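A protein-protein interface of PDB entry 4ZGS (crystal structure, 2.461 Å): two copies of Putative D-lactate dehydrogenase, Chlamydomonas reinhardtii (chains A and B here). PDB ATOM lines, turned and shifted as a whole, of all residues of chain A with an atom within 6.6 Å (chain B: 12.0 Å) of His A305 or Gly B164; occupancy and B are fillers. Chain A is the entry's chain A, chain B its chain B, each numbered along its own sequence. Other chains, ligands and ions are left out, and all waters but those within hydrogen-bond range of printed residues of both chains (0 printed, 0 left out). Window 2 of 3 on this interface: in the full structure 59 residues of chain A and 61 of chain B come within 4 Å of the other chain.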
ATOM      1  N   GLY A 299      10.620   6.343  17.798  1.00  0.00           N
ATOM      2  CA  GLY A 299      10.107   7.685  17.979  1.00  0.00           C
ATOM      3  C   GLY A 299      10.697   8.639  16.953  1.00  0.00           C
ATOM      4  O   GLY A 299      10.163   9.727  16.733  1.00  0.00           O
ATOM      5  N   LEU A 300      11.786   8.230  16.305  1.00  0.00           N
ATOM      6  CA  LEU A 300      12.466   9.065  15.306  1.00  0.00           C
ATOM      7  C   LEU A 300      11.910   8.859  13.886  1.00  0.00           C
ATOM      8  O   LEU A 300      11.463   9.810  13.242  1.00  0.00           O
ATOM      9  CB  LEU A 300      13.976   8.805  15.326  1.00  0.00           C
ATOM     10  CG  LEU A 300      14.876   9.699  14.462  1.00  0.00           C
ATOM     11  CD1 LEU A 300      14.792  11.166  14.872  1.00  0.00           C
ATOM     12  CD2 LEU A 300      16.337   9.203  14.441  1.00  0.00           C
ATOM     13  N   PHE A 301      11.996   7.643  13.363  1.00  0.00           N
ATOM     14  CA  PHE A 301      11.522   7.395  11.997  1.00  0.00           C
ATOM     15  C   PHE A 301       9.991   7.280  11.828  1.00  0.00           C
ATOM     16  O   PHE A 301       9.241   7.038  12.776  1.00  0.00           O
ATOM     17  CB  PHE A 301      12.192   6.156  11.418  1.00  0.00           C
ATOM     18  CG  PHE A 301      13.560   6.410  10.853  1.00  0.00           C
ATOM     19  CD1 PHE A 301      14.563   6.964  11.633  1.00  0.00           C
ATOM     20  CD2 PHE A 301      13.845   6.102   9.522  1.00  0.00           C
ATOM     21  CE1 PHE A 301      15.843   7.193  11.095  1.00  0.00           C
ATOM     22  CE2 PHE A 301      15.116   6.323   8.981  1.00  0.00           C
ATOM     23  CZ  PHE A 301      16.114   6.869   9.769  1.00  0.00           C
ATOM     24  N   PHE A 302       9.556   7.459  10.586  1.00  0.00           N
ATOM     25  CA  PHE A 302       8.145   7.413  10.210  1.00  0.00           C
ATOM     26  C   PHE A 302       7.312   8.539  10.827  1.00  0.00           C
ATOM     27  O   PHE A 302       6.086   8.487  10.838  1.00  0.00           O
ATOM     28  CB  PHE A 302       7.527   6.086  10.633  1.00  0.00           C
ATOM     29  CG  PHE A 302       8.347   4.873  10.301  1.00  0.00           C
ATOM     30  CD1 PHE A 302       8.478   4.442   8.990  1.00  0.00           C
ATOM     31  CD2 PHE A 302       8.939   4.130  11.313  1.00  0.00           C
ATOM     32  CE1 PHE A 302       9.208   3.309   8.693  1.00  0.00           C
ATOM     33  CE2 PHE A 302       9.661   2.989  11.026  1.00  0.00           C
ATOM     34  CZ  PHE A 302       9.799   2.573   9.714  1.00  0.00           C
ATOM     35  N   VAL A 303       7.984   9.587  11.264  1.00  0.00           N
ATOM     36  CA  VAL A 303       7.319  10.761  11.792  1.00  0.00           C
ATOM     37  C   VAL A 303       7.839  11.989  11.056  1.00  0.00           C
ATOM     38  O   VAL A 303       9.043  12.101  10.801  1.00  0.00           O
ATOM     39  CB  VAL A 303       7.566  10.967  13.283  1.00  0.00           C
ATOM     40  CG1 VAL A 303       6.963  12.300  13.701  1.00  0.00           C
ATOM     41  CG2 VAL A 303       6.988   9.829  14.104  1.00  0.00           C
ATOM     42  N   ASP A 304       6.942  12.901  10.701  1.00  0.00           N
ATOM     43  CA  ASP A 304       7.406  14.179  10.221  1.00  0.00           C
ATOM     44  C   ASP A 304       7.481  15.128  11.406  1.00  0.00           C
ATOM     45  O   ASP A 304       6.476  15.662  11.837  1.00  0.00           O
ATOM     46  CB  ASP A 304       6.463  14.747   9.157  1.00  0.00           C
ATOM     47  CG  ASP A 304       6.825  16.178   8.768  1.00  0.00           C
ATOM     48  OD1 ASP A 304       7.919  16.667   9.133  1.00  0.00           O
ATOM     49  OD2 ASP A 304       5.999  16.836   8.116  1.00  0.00           O
ATOM     50  N   HIS A 305       8.688  15.410  11.865  1.00  0.00           N
ATOM     51  CA  HIS A 305       8.872  16.265  13.040  1.00  0.00           C
ATOM     52  C   HIS A 305       8.713  17.746  12.703  1.00  0.00           C
ATOM     53  O   HIS A 305       8.719  18.562  13.607  1.00  0.00           O
ATOM     54  CB  HIS A 305      10.240  16.030  13.683  1.00  0.00           C
ATOM     55  CG  HIS A 305      10.445  14.616  14.130  1.00  0.00           C
ATOM     56  ND1 HIS A 305       9.913  14.120  15.299  1.00  0.00           N
ATOM     57  CD2 HIS A 305      11.117  13.589  13.558  1.00  0.00           C
ATOM     58  CE1 HIS A 305      10.244  12.847  15.432  1.00  0.00           C
ATOM     59  NE2 HIS A 305      10.980  12.502  14.392  1.00  0.00           N
ATOM     60  N   THR A 306       8.604  18.085  11.420  1.00  0.00           N
ATOM     61  CA  THR A 306       8.420  19.467  10.992  1.00  0.00           C
ATOM     62  C   THR A 306       7.011  19.982  11.326  1.00  0.00           C
ATOM     63  O   THR A 306       6.732  21.182  11.228  1.00  0.00           O
ATOM     64  CB  THR A 306       8.652  19.678   9.488  1.00  0.00           C
ATOM     65  OG1 THR A 306       7.533  19.154   8.754  1.00  0.00           O
ATOM     66  CG2 THR A 306       9.931  19.042   9.049  1.00  0.00           C
ATOM     67  N   LYS A 307       6.119  19.076  11.678  1.00  0.00           N
ATOM     68  CA  LYS A 307       4.773  19.489  12.049  1.00  0.00           C
ATOM     69  C   LYS A 307       4.720  19.968  13.502  1.00  0.00           C
ATOM     70  O   LYS A 307       3.750  20.555  13.911  1.00  0.00           O
ATOM     71  CB  LYS A 307       3.794  18.337  11.809  1.00  0.00           C
ATOM     72  CG  LYS A 307       3.975  17.152  12.750  1.00  0.00           C
ATOM     73  CD  LYS A 307       3.059  16.000  12.311  1.00  0.00           C
ATOM     74  CE  LYS A 307       3.352  14.679  13.018  1.00  0.00           C
ATOM     75  NZ  LYS A 307       2.883  14.666  14.425  1.00  0.00           N
ATOM     76  N   PHE A 308       5.774  19.730  14.267  1.00  0.00           N
ATOM     77  CA  PHE A 308       5.815  20.149  15.667  1.00  0.00           C
ATOM     78  C   PHE A 308       6.550  21.501  15.835  1.00  0.00           C
ATOM     79  O   PHE A 308       7.512  21.826  15.104  1.00  0.00           O
ATOM     80  CB  PHE A 308       6.510  19.095  16.535  1.00  0.00           C
ATOM     81  CG  PHE A 308       5.819  17.747  16.567  1.00  0.00           C
ATOM     82  CD1 PHE A 308       4.654  17.547  17.291  1.00  0.00           C
ATOM     83  CD2 PHE A 308       6.362  16.659  15.849  1.00  0.00           C
ATOM     84  CE1 PHE A 308       4.035  16.276  17.314  1.00  0.00           C
ATOM     85  CE2 PHE A 308       5.769  15.422  15.873  1.00  0.00           C
ATOM     86  CZ  PHE A 308       4.608  15.227  16.600  1.00  0.00           C
ATOM     87  N   ASP A 309       6.112  22.286  16.808  1.00  0.00           N
ATOM     88  CA  ASP A 309       6.895  23.440  17.207  1.00  0.00           C
ATOM     89  C   ASP A 309       8.298  23.008  17.609  1.00  0.00           C
ATOM     90  O   ASP A 309       8.462  21.996  18.289  1.00  0.00           O
ATOM     91  CB  ASP A 309       6.234  24.157  18.375  1.00  0.00           C
ATOM     92  CG  ASP A 309       7.007  25.376  18.801  1.00  0.00           C
ATOM     93  OD1 ASP A 309       6.739  26.458  18.231  1.00  0.00           O
ATOM     94  OD2 ASP A 309       7.901  25.242  19.670  1.00  0.00           O
ATOM     95  N   PRO A 310       9.314  23.804  17.239  1.00  0.00           N
ATOM     96  CA  PRO A 310      10.717  23.467  17.524  1.00  0.00           C
ATOM     97  C   PRO A 310      10.949  23.161  19.009  1.00  0.00           C
ATOM     98  O   PRO A 310      11.777  22.326  19.370  1.00  0.00           O
ATOM     99  CB  PRO A 310      11.478  24.728  17.079  1.00  0.00           C
ATOM    100  CG  PRO A 310      10.610  25.348  16.021  1.00  0.00           C
ATOM    101  CD  PRO A 310       9.188  25.071  16.488  1.00  0.00           C
ATOM    102  N   ARG A 313       9.999  19.717  19.386  1.00  0.00           N
ATOM    103  CA  ARG A 313      11.038  18.943  18.726  1.00  0.00           C
ATOM    104  C   ARG A 313      12.290  18.823  19.606  1.00  0.00           C
ATOM    105  O   ARG A 313      12.976  17.799  19.546  1.00  0.00           O
ATOM    106  CB  ARG A 313      11.396  19.560  17.367  1.00  0.00           C
ATOM    107  CG  ARG A 313      10.259  19.573  16.331  1.00  0.00           C
ATOM    108  CD  ARG A 313      10.705  20.306  15.041  1.00  0.00           C
ATOM    109  NE  ARG A 313      11.781  19.600  14.343  1.00  0.00           N
ATOM    110  CZ  ARG A 313      12.255  19.935  13.141  1.00  0.00           C
ATOM    111  NH1 ARG A 313      11.734  20.964  12.474  1.00  0.00           N
ATOM    112  NH2 ARG A 313      13.234  19.212  12.590  1.00  0.00           N
ATOM    113  N   LYS A 316      12.805  15.279  22.042  1.00  0.00           N
ATOM    114  CA  LYS A 316      13.440  14.064  21.523  1.00  0.00           C
ATOM    115  C   LYS A 316      14.645  14.320  20.619  1.00  0.00           C
ATOM    116  O   LYS A 316      15.040  13.423  19.878  1.00  0.00           O
ATOM    117  CB  LYS A 316      12.442  13.157  20.790  1.00  0.00           C
ATOM    118  CG  LYS A 316      11.501  12.385  21.736  1.00  0.00           C
ATOM    119  CD  LYS A 316      10.616  11.375  20.981  1.00  0.00           C
ATOM    120  CE  LYS A 316       9.683  11.997  19.945  1.00  0.00           C
ATOM    121  NZ  LYS A 316       8.828  10.946  19.296  1.00  0.00           N
ATOM    122  N   ARG A 322      21.379  14.450  13.835  1.00  0.00           N
ATOM    123  CA  ARG A 322      21.274  15.731  13.113  1.00  0.00           C
ATOM    124  C   ARG A 322      22.659  16.224  12.639  1.00  0.00           C
ATOM    125  O   ARG A 322      22.819  16.799  11.548  1.00  0.00           O
ATOM    126  CB  ARG A 322      20.579  16.789  14.006  1.00  0.00           C
ATOM    127  CG  ARG A 322      19.117  16.442  14.435  1.00  0.00           C
ATOM    128  CD  ARG A 322      18.232  16.263  13.194  1.00  0.00           C
ATOM    129  NE  ARG A 322      18.071  17.515  12.452  1.00  0.00           N
ATOM    130  CZ  ARG A 322      17.558  17.611  11.223  1.00  0.00           C
ATOM    131  NH1 ARG A 322      17.163  16.526  10.552  1.00  0.00           N
ATOM    132  NH2 ARG A 322      17.466  18.800  10.647  1.00  0.00           N
ATOM    133  N   LEU A 325      23.751  14.181   9.498  1.00  0.00           N
ATOM    134  CA  LEU A 325      23.080  14.727   8.321  1.00  0.00           C
ATOM    135  C   LEU A 325      23.786  15.977   7.791  1.00  0.00           C
ATOM    136  O   LEU A 325      23.460  16.480   6.721  1.00  0.00           O
ATOM    137  CB  LEU A 325      21.630  15.044   8.667  1.00  0.00           C
ATOM    138  CG  LEU A 325      20.829  13.842   9.168  1.00  0.00           C
ATOM    139  CD1 LEU A 325      19.481  14.289   9.652  1.00  0.00           C
ATOM    140  CD2 LEU A 325      20.663  12.794   8.034  1.00  0.00           C
ATOM    141  N   THR B 155      16.144  12.512  -4.193  1.00  0.00           N
ATOM    142  CA  THR B 155      16.319  13.926  -3.928  1.00  0.00           C
ATOM    143  C   THR B 155      15.267  14.409  -2.900  1.00  0.00           C
ATOM    144  O   THR B 155      15.637  15.022  -1.882  1.00  0.00           O
ATOM    145  CB  THR B 155      16.259  14.778  -5.228  1.00  0.00           C
ATOM    146  OG1 THR B 155      14.984  14.640  -5.861  1.00  0.00           O
ATOM    147  CG2 THR B 155      17.356  14.374  -6.215  1.00  0.00           C
ATOM    148  N   ASP B 156      13.997  14.065  -3.138  1.00  0.00           N
ATOM    149  CA  ASP B 156      12.893  14.252  -2.178  1.00  0.00           C
ATOM    150  C   ASP B 156      13.256  13.747  -0.797  1.00  0.00           C
ATOM    151  O   ASP B 156      13.065  14.432   0.223  1.00  0.00           O
ATOM    152  CB  ASP B 156      11.642  13.522  -2.650  1.00  0.00           C
ATOM    153  CG  ASP B 156      11.049  14.120  -3.896  1.00  0.00           C
ATOM    154  OD1 ASP B 156      11.120  15.360  -4.004  1.00  0.00           O
ATOM    155  OD2 ASP B 156      10.539  13.362  -4.768  1.00  0.00           O
ATOM    156  N   ALA B 157      13.753  12.524  -0.743  1.00  0.00           N
ATOM    157  CA  ALA B 157      14.002  11.913   0.558  1.00  0.00           C
ATOM    158  C   ALA B 157      15.095  12.667   1.309  1.00  0.00           C
ATOM    159  O   ALA B 157      15.011  12.848   2.515  1.00  0.00           O
ATOM    160  CB  ALA B 157      14.358  10.431   0.407  1.00  0.00           C
ATOM    161  N   TYR B 158      16.142  13.046   0.591  1.00  0.00           N
ATOM    162  CA  TYR B 158      17.275  13.731   1.168  1.00  0.00           C
ATOM    163  C   TYR B 158      16.882  15.030   1.832  1.00  0.00           C
ATOM    164  O   TYR B 158      17.285  15.302   2.964  1.00  0.00           O
ATOM    165  CB  TYR B 158      18.322  14.020   0.100  1.00  0.00           C
ATOM    166  CG  TYR B 158      19.482  14.858   0.595  1.00  0.00           C
ATOM    167  CD1 TYR B 158      20.432  14.330   1.462  1.00  0.00           C
ATOM    168  CD2 TYR B 158      19.632  16.178   0.184  1.00  0.00           C
ATOM    169  CE1 TYR B 158      21.516  15.113   1.928  1.00  0.00           C
ATOM    170  CE2 TYR B 158      20.704  16.962   0.634  1.00  0.00           C
ATOM    171  CZ  TYR B 158      21.644  16.425   1.507  1.00  0.00           C
ATOM    172  OH  TYR B 158      22.715  17.208   1.946  1.00  0.00           O
ATOM    173  N   ILE B 159      16.123  15.834   1.094  1.00  0.00           N
ATOM    174  CA  ILE B 159      15.734  17.162   1.552  1.00  0.00           C
ATOM    175  C   ILE B 159      14.785  17.082   2.763  1.00  0.00           C
ATOM    176  O   ILE B 159      14.959  17.805   3.764  1.00  0.00           O
ATOM    177  CB  ILE B 159      15.070  17.976   0.417  1.00  0.00           C
ATOM    178  CG1 ILE B 159      16.108  18.434  -0.600  1.00  0.00           C
ATOM    179  CG2 ILE B 159      14.408  19.223   0.961  1.00  0.00           C
ATOM    180  CD1 ILE B 159      15.483  18.976  -1.888  1.00  0.00           C
ATOM    181  N   ARG B 160      13.797  16.197   2.672  1.00  0.00           N
ATOM    182  CA  ARG B 160      12.859  16.028   3.771  1.00  0.00           C
ATOM    183  C   ARG B 160      13.560  15.631   5.038  1.00  0.00           C
ATOM    184  O   ARG B 160      13.318  16.207   6.109  1.00  0.00           O
ATOM    185  CB  ARG B 160      11.837  14.995   3.450  1.00  0.00           C
ATOM    186  CG  ARG B 160      10.844  15.299   2.362  1.00  0.00           C
ATOM    187  CD  ARG B 160      10.234  13.895   2.260  1.00  0.00           C
ATOM    188  NE  ARG B 160       8.980  13.782   1.567  1.00  0.00           N
ATOM    189  CZ  ARG B 160       8.016  12.994   1.999  1.00  0.00           C
ATOM    190  NH1 ARG B 160       8.194  12.294   3.115  1.00  0.00           N
ATOM    191  NH2 ARG B 160       6.881  12.903   1.315  1.00  0.00           N
ATOM    192  N   VAL B 161      14.417  14.629   4.895  1.00  0.00           N
ATOM    193  CA  VAL B 161      15.228  14.160   6.005  1.00  0.00           C
ATOM    194  C   VAL B 161      16.123  15.280   6.547  1.00  0.00           C
ATOM    195  O   VAL B 161      16.332  15.378   7.764  1.00  0.00           O
ATOM    196  CB  VAL B 161      16.082  12.971   5.575  1.00  0.00           C
ATOM    197  CG1 VAL B 161      17.053  12.555   6.694  1.00  0.00           C
ATOM    198  CG2 VAL B 161      15.162  11.825   5.201  1.00  0.00           C
ATOM    199  N   ARG B 162      16.630  16.135   5.656  1.00  0.00           N
ATOM    200  CA  ARG B 162      17.454  17.236   6.124  1.00  0.00           C
ATOM    201  C   ARG B 162      16.571  18.163   6.957  1.00  0.00           C
ATOM    202  O   ARG B 162      17.033  18.685   7.966  1.00  0.00           O
ATOM    203  CB  ARG B 162      18.153  18.008   4.988  1.00  0.00           C
ATOM    204  CG  ARG B 162      19.293  17.265   4.304  1.00  0.00           C
ATOM    205  CD  ARG B 162      20.616  17.299   5.083  1.00  0.00           C
ATOM    206  NE  ARG B 162      21.067  18.624   5.541  1.00  0.00           N
ATOM    207  CZ  ARG B 162      21.849  19.468   4.857  1.00  0.00           C
ATOM    208  NH1 ARG B 162      22.265  19.176   3.630  1.00  0.00           N
ATOM    209  NH2 ARG B 162      22.206  20.625   5.402  1.00  0.00           N
ATOM    210  N   MET B 163      15.310  18.333   6.547  1.00  0.00           N
ATOM    211  CA  MET B 163      14.332  19.124   7.321  1.00  0.00           C
ATOM    212  C   MET B 163      13.850  18.429   8.578  1.00  0.00           C
ATOM    213  O   MET B 163      13.361  19.070   9.491  1.00  0.00           O
ATOM    214  CB  MET B 163      13.094  19.473   6.480  1.00  0.00           C
ATOM    215  CG  MET B 163      13.357  20.198   5.157  1.00  0.00           C
ATOM    216  SD  MET B 163      11.841  20.568   4.249  1.00  0.00           S
ATOM    217  CE  MET B 163      10.815  19.157   4.664  1.00  0.00           C
ATOM    218  N   GLY B 164      13.956  17.109   8.632  1.00  0.00           N
ATOM    219  CA  GLY B 164      13.438  16.365   9.776  1.00  0.00           C
ATOM    220  C   GLY B 164      12.049  15.788   9.545  1.00  0.00           C
ATOM    221  O   GLY B 164      11.366  15.404  10.492  1.00  0.00           O
ATOM    222  N   ASN B 165      11.621  15.731   8.285  1.00  0.00           N
ATOM    223  CA  ASN B 165      10.457  14.929   7.905  1.00  0.00           C
ATOM    224  C   ASN B 165      10.987  13.584   7.512  1.00  0.00           C
ATOM    225  O   ASN B 165      11.538  13.430   6.437  1.00  0.00           O
ATOM    226  CB  ASN B 165       9.691  15.570   6.733  1.00  0.00           C
ATOM    227  CG  ASN B 165       8.500  14.754   6.253  1.00  0.00           C
ATOM    228  OD1 ASN B 165       8.199  13.653   6.752  1.00  0.00           O
ATOM    229  ND2 ASN B 165       7.780  15.320   5.289  1.00  0.00           N
ATOM    230  N   TYR B 166      10.786  12.624   8.405  1.00  0.00           N
ATOM    231  CA  TYR B 166      11.134  11.207   8.261  1.00  0.00           C
ATOM    232  C   TYR B 166       9.884  10.352   7.891  1.00  0.00           C
ATOM    233  O   TYR B 166       9.880   9.137   8.076  1.00  0.00           O
ATOM    234  CB  TYR B 166      11.799  10.683   9.544  1.00  0.00           C
ATOM    235  CG  TYR B 166      12.910  11.565  10.101  1.00  0.00           C
ATOM    236  CD1 TYR B 166      13.726  12.324   9.266  1.00  0.00           C
ATOM    237  CD2 TYR B 166      13.134  11.639  11.469  1.00  0.00           C
ATOM    238  CE1 TYR B 166      14.749  13.129   9.781  1.00  0.00           C
ATOM    239  CE2 TYR B 166      14.136  12.439  12.000  1.00  0.00           C
ATOM    240  CZ  TYR B 166      14.948  13.186  11.153  1.00  0.00           C
ATOM    241  OH  TYR B 166      15.948  13.981  11.695  1.00  0.00           O
ATOM    242  N   SER B 167       8.772  10.984   7.516  1.00  0.00           N
ATOM    243  CA  SER B 167       7.586  10.198   7.135  1.00  0.00           C
ATOM    244  C   SER B 167       7.755   9.516   5.762  1.00  0.00           C
ATOM    245  O   SER B 167       8.597   9.940   4.938  1.00  0.00           O
ATOM    246  CB  SER B 167       6.346  11.083   7.153  1.00  0.00           C
ATOM    247  OG  SER B 167       6.365  11.958   6.039  1.00  0.00           O
ATOM    248  N   LEU B 168       6.983   8.449   5.525  1.00  0.00           N
ATOM    249  CA  LEU B 168       7.136   7.618   4.305  1.00  0.00           C
ATOM    250  C   LEU B 168       6.401   8.107   3.055  1.00  0.00           C
ATOM    251  O   LEU B 168       6.918   7.944   1.945  1.00  0.00           O
ATOM    252  CB  LEU B 168       6.727   6.186   4.589  1.00  0.00           C
ATOM    253  CG  LEU B 168       7.620   5.510   5.632  1.00  0.00           C
ATOM    254  CD1 LEU B 168       7.246   4.041   5.826  1.00  0.00           C
ATOM    255  CD2 LEU B 168       9.071   5.627   5.180  1.00  0.00           C
ATOM    256  N   SER B 169       5.204   8.657   3.191  1.00  0.00           N
ATOM    257  CA  SER B 169       4.481   9.145   2.016  1.00  0.00           C
ATOM    258  C   SER B 169       5.302  10.288   1.502  1.00  0.00           C
ATOM    259  O   SER B 169       5.989  10.900   2.326  1.00  0.00           O
ATOM    260  CB  SER B 169       3.081   9.635   2.412  1.00  0.00           C
ATOM    261  OG  SER B 169       2.537   8.835   3.441  1.00  0.00           O
ATOM    262  N   LEU B 171       7.247   9.036  -0.834  1.00  0.00           N
ATOM    263  CA  LEU B 171       8.513   8.474  -1.268  1.00  0.00           C
ATOM    264  C   LEU B 171       8.412   7.041  -1.906  1.00  0.00           C
ATOM    265  O   LEU B 171       9.419   6.387  -2.105  1.00  0.00           O
ATOM    266  CB  LEU B 171       9.480   8.443  -0.077  1.00  0.00           C
ATOM    267  CG  LEU B 171       9.700   9.789   0.629  1.00  0.00           C
ATOM    268  CD1 LEU B 171      10.778   9.638   1.709  1.00  0.00           C
ATOM    269  CD2 LEU B 171      10.013  10.876  -0.369  1.00  0.00           C
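No position is printed for both chains.
Of the 16 printed residues of chain B, 8 touch a printed residue of chain A.
Hydrophobic or aromatic side chains of chain B that line the printed part of chain A: Val B161, Tyr B166 and Leu B168.
Hydrophobic or aromatic side chains of chain A within 4 Å of the printed part of chain B: Leu A300, Phe A302, His A305 and Leu A325.
O of Tyr B166 sits at hydrogen-bond distance from N of Phe A302 (3.0 Å).
NH2 of Arg A313 lies within hydrogen-bond range of O of Met B163.
NH2 of Arg A322 is in hydrogen-bond range of O of Arg B162.
The backbone carbonyl oxygen (O) of Val A303 sits at hydrogen-bond distance from the backbone NH (N) of Tyr B166, at 3.0 Å.
O of Gly B164 is in hydrogen-bond range of N of His A305 (3.0 Å).
The backbone carbonyl oxygen of Val B161 is in hydrogen-bond range of the guanidinium group of Arg A322, at 3.1 Å.
O of Val A303 sits at hydrogen-bond distance from N of Ser B167.
OH of Tyr B166 sits at hydrogen-bond distance from NH1 of Arg A322 (3.0 Å).
The backbone carbonyl oxygen (O) of Leu A325 lies close to the guanidinium group (NE) of Arg B162, 3.4 Å away.
The side-chain carboxylate of Asp A304 sits at hydrogen-bond distance from the side-chain hydroxyl of Thr A306, at 2.5 Å.
The guanidinium group (NH1) of Arg B160 is in hydrogen-bond range of the backbone carbonyl oxygen (O) of Ser B167 (3.0 Å).
The guanidinium group of Arg B162 sits at hydrogen-bond distance from the side-chain hydroxyl of Tyr B158 (2.6 Å).
A ring nitrogen (NE2) of His A305 lies within hydrogen-bond range of the backbone carbonyl oxygen of Leu A300, 3.0 Å away.
The side-chain hydroxyl (OG) of Ser B167 is in hydrogen-bond range of the side-chain amide oxygen (OD1) of Asn B165 (2.6 Å).
O of Arg B160 sits at hydrogen-bond distance from N of Asn B165, 2.8 Å away.
Tyr B166 touches Leu A300.
Phe A302 touches Leu B168 (CD1 to CD1, 3.4 Å).
O of Gly B164 touches OD1 of Asp A304 (3.9 Å).
OD1 of Asn B165 touches CB of Asp A304, 3.2 Å away.
CD2 of His A305 touches CD2 of Tyr B166, 3.5 Å away.
Thr A306 touches Met B163 (CG2 to O, 3.5 Å).
CG2 of Thr A306 touches C of Gly B164, at 3.9 Å.
Thr A306 touches Asn B165.
NH1 of Arg A322 touches N of Gly B164 (3.8 Å).
O of Val B161 touches CD1 of Leu A325 (3.8 Å).
His A305 touches just these residues of chain B: Gly B164 and Tyr B166.
Printed residues of chain A within 4 Å of Gly B164: Asp A304, His A305, Thr A306 and Arg A322.
Gly A299 touches none of the printed residues of chain B.
Leu A300 touches just one residue of chain B: Tyr B166 (3.0 Å).
Of chain B, only Tyr B166 and Ser B167 come within 4 Å of Val A303.
Asp A304 touches two residues of chain B.
Of chain B, only Met B163 (3.5 Å), Gly B164 (3.9 Å) and Asn B165 (3.8 Å) come within 4 Å of Thr A306.
No residue of chain B comes within 4 Å of Phe A308.
No residue of chain B comes within 4 Å of Lys A316.
Of the printed residues of chain A, Leu B168 touches Phe A302 (3.4 Å).
Of the printed residues of chain A, Arg B162 touches Arg A322 (2.7 Å) and Leu A325 (3.4 Å).
Printed residues of chain A within 4 Å of Tyr B166: Leu A300, Phe A302, Val A303, His A305 and Arg A322.
The nearest residue of chain B that does not touch His A305 is Asn B165 (4.4 Å).
The nearest printed residue of chain A that does not touch Gly B164 is Arg A313 (4.01 Å).
The nearest printed residue of chain A that does not touch Val B161 is Phe A301 (6.5 Å).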
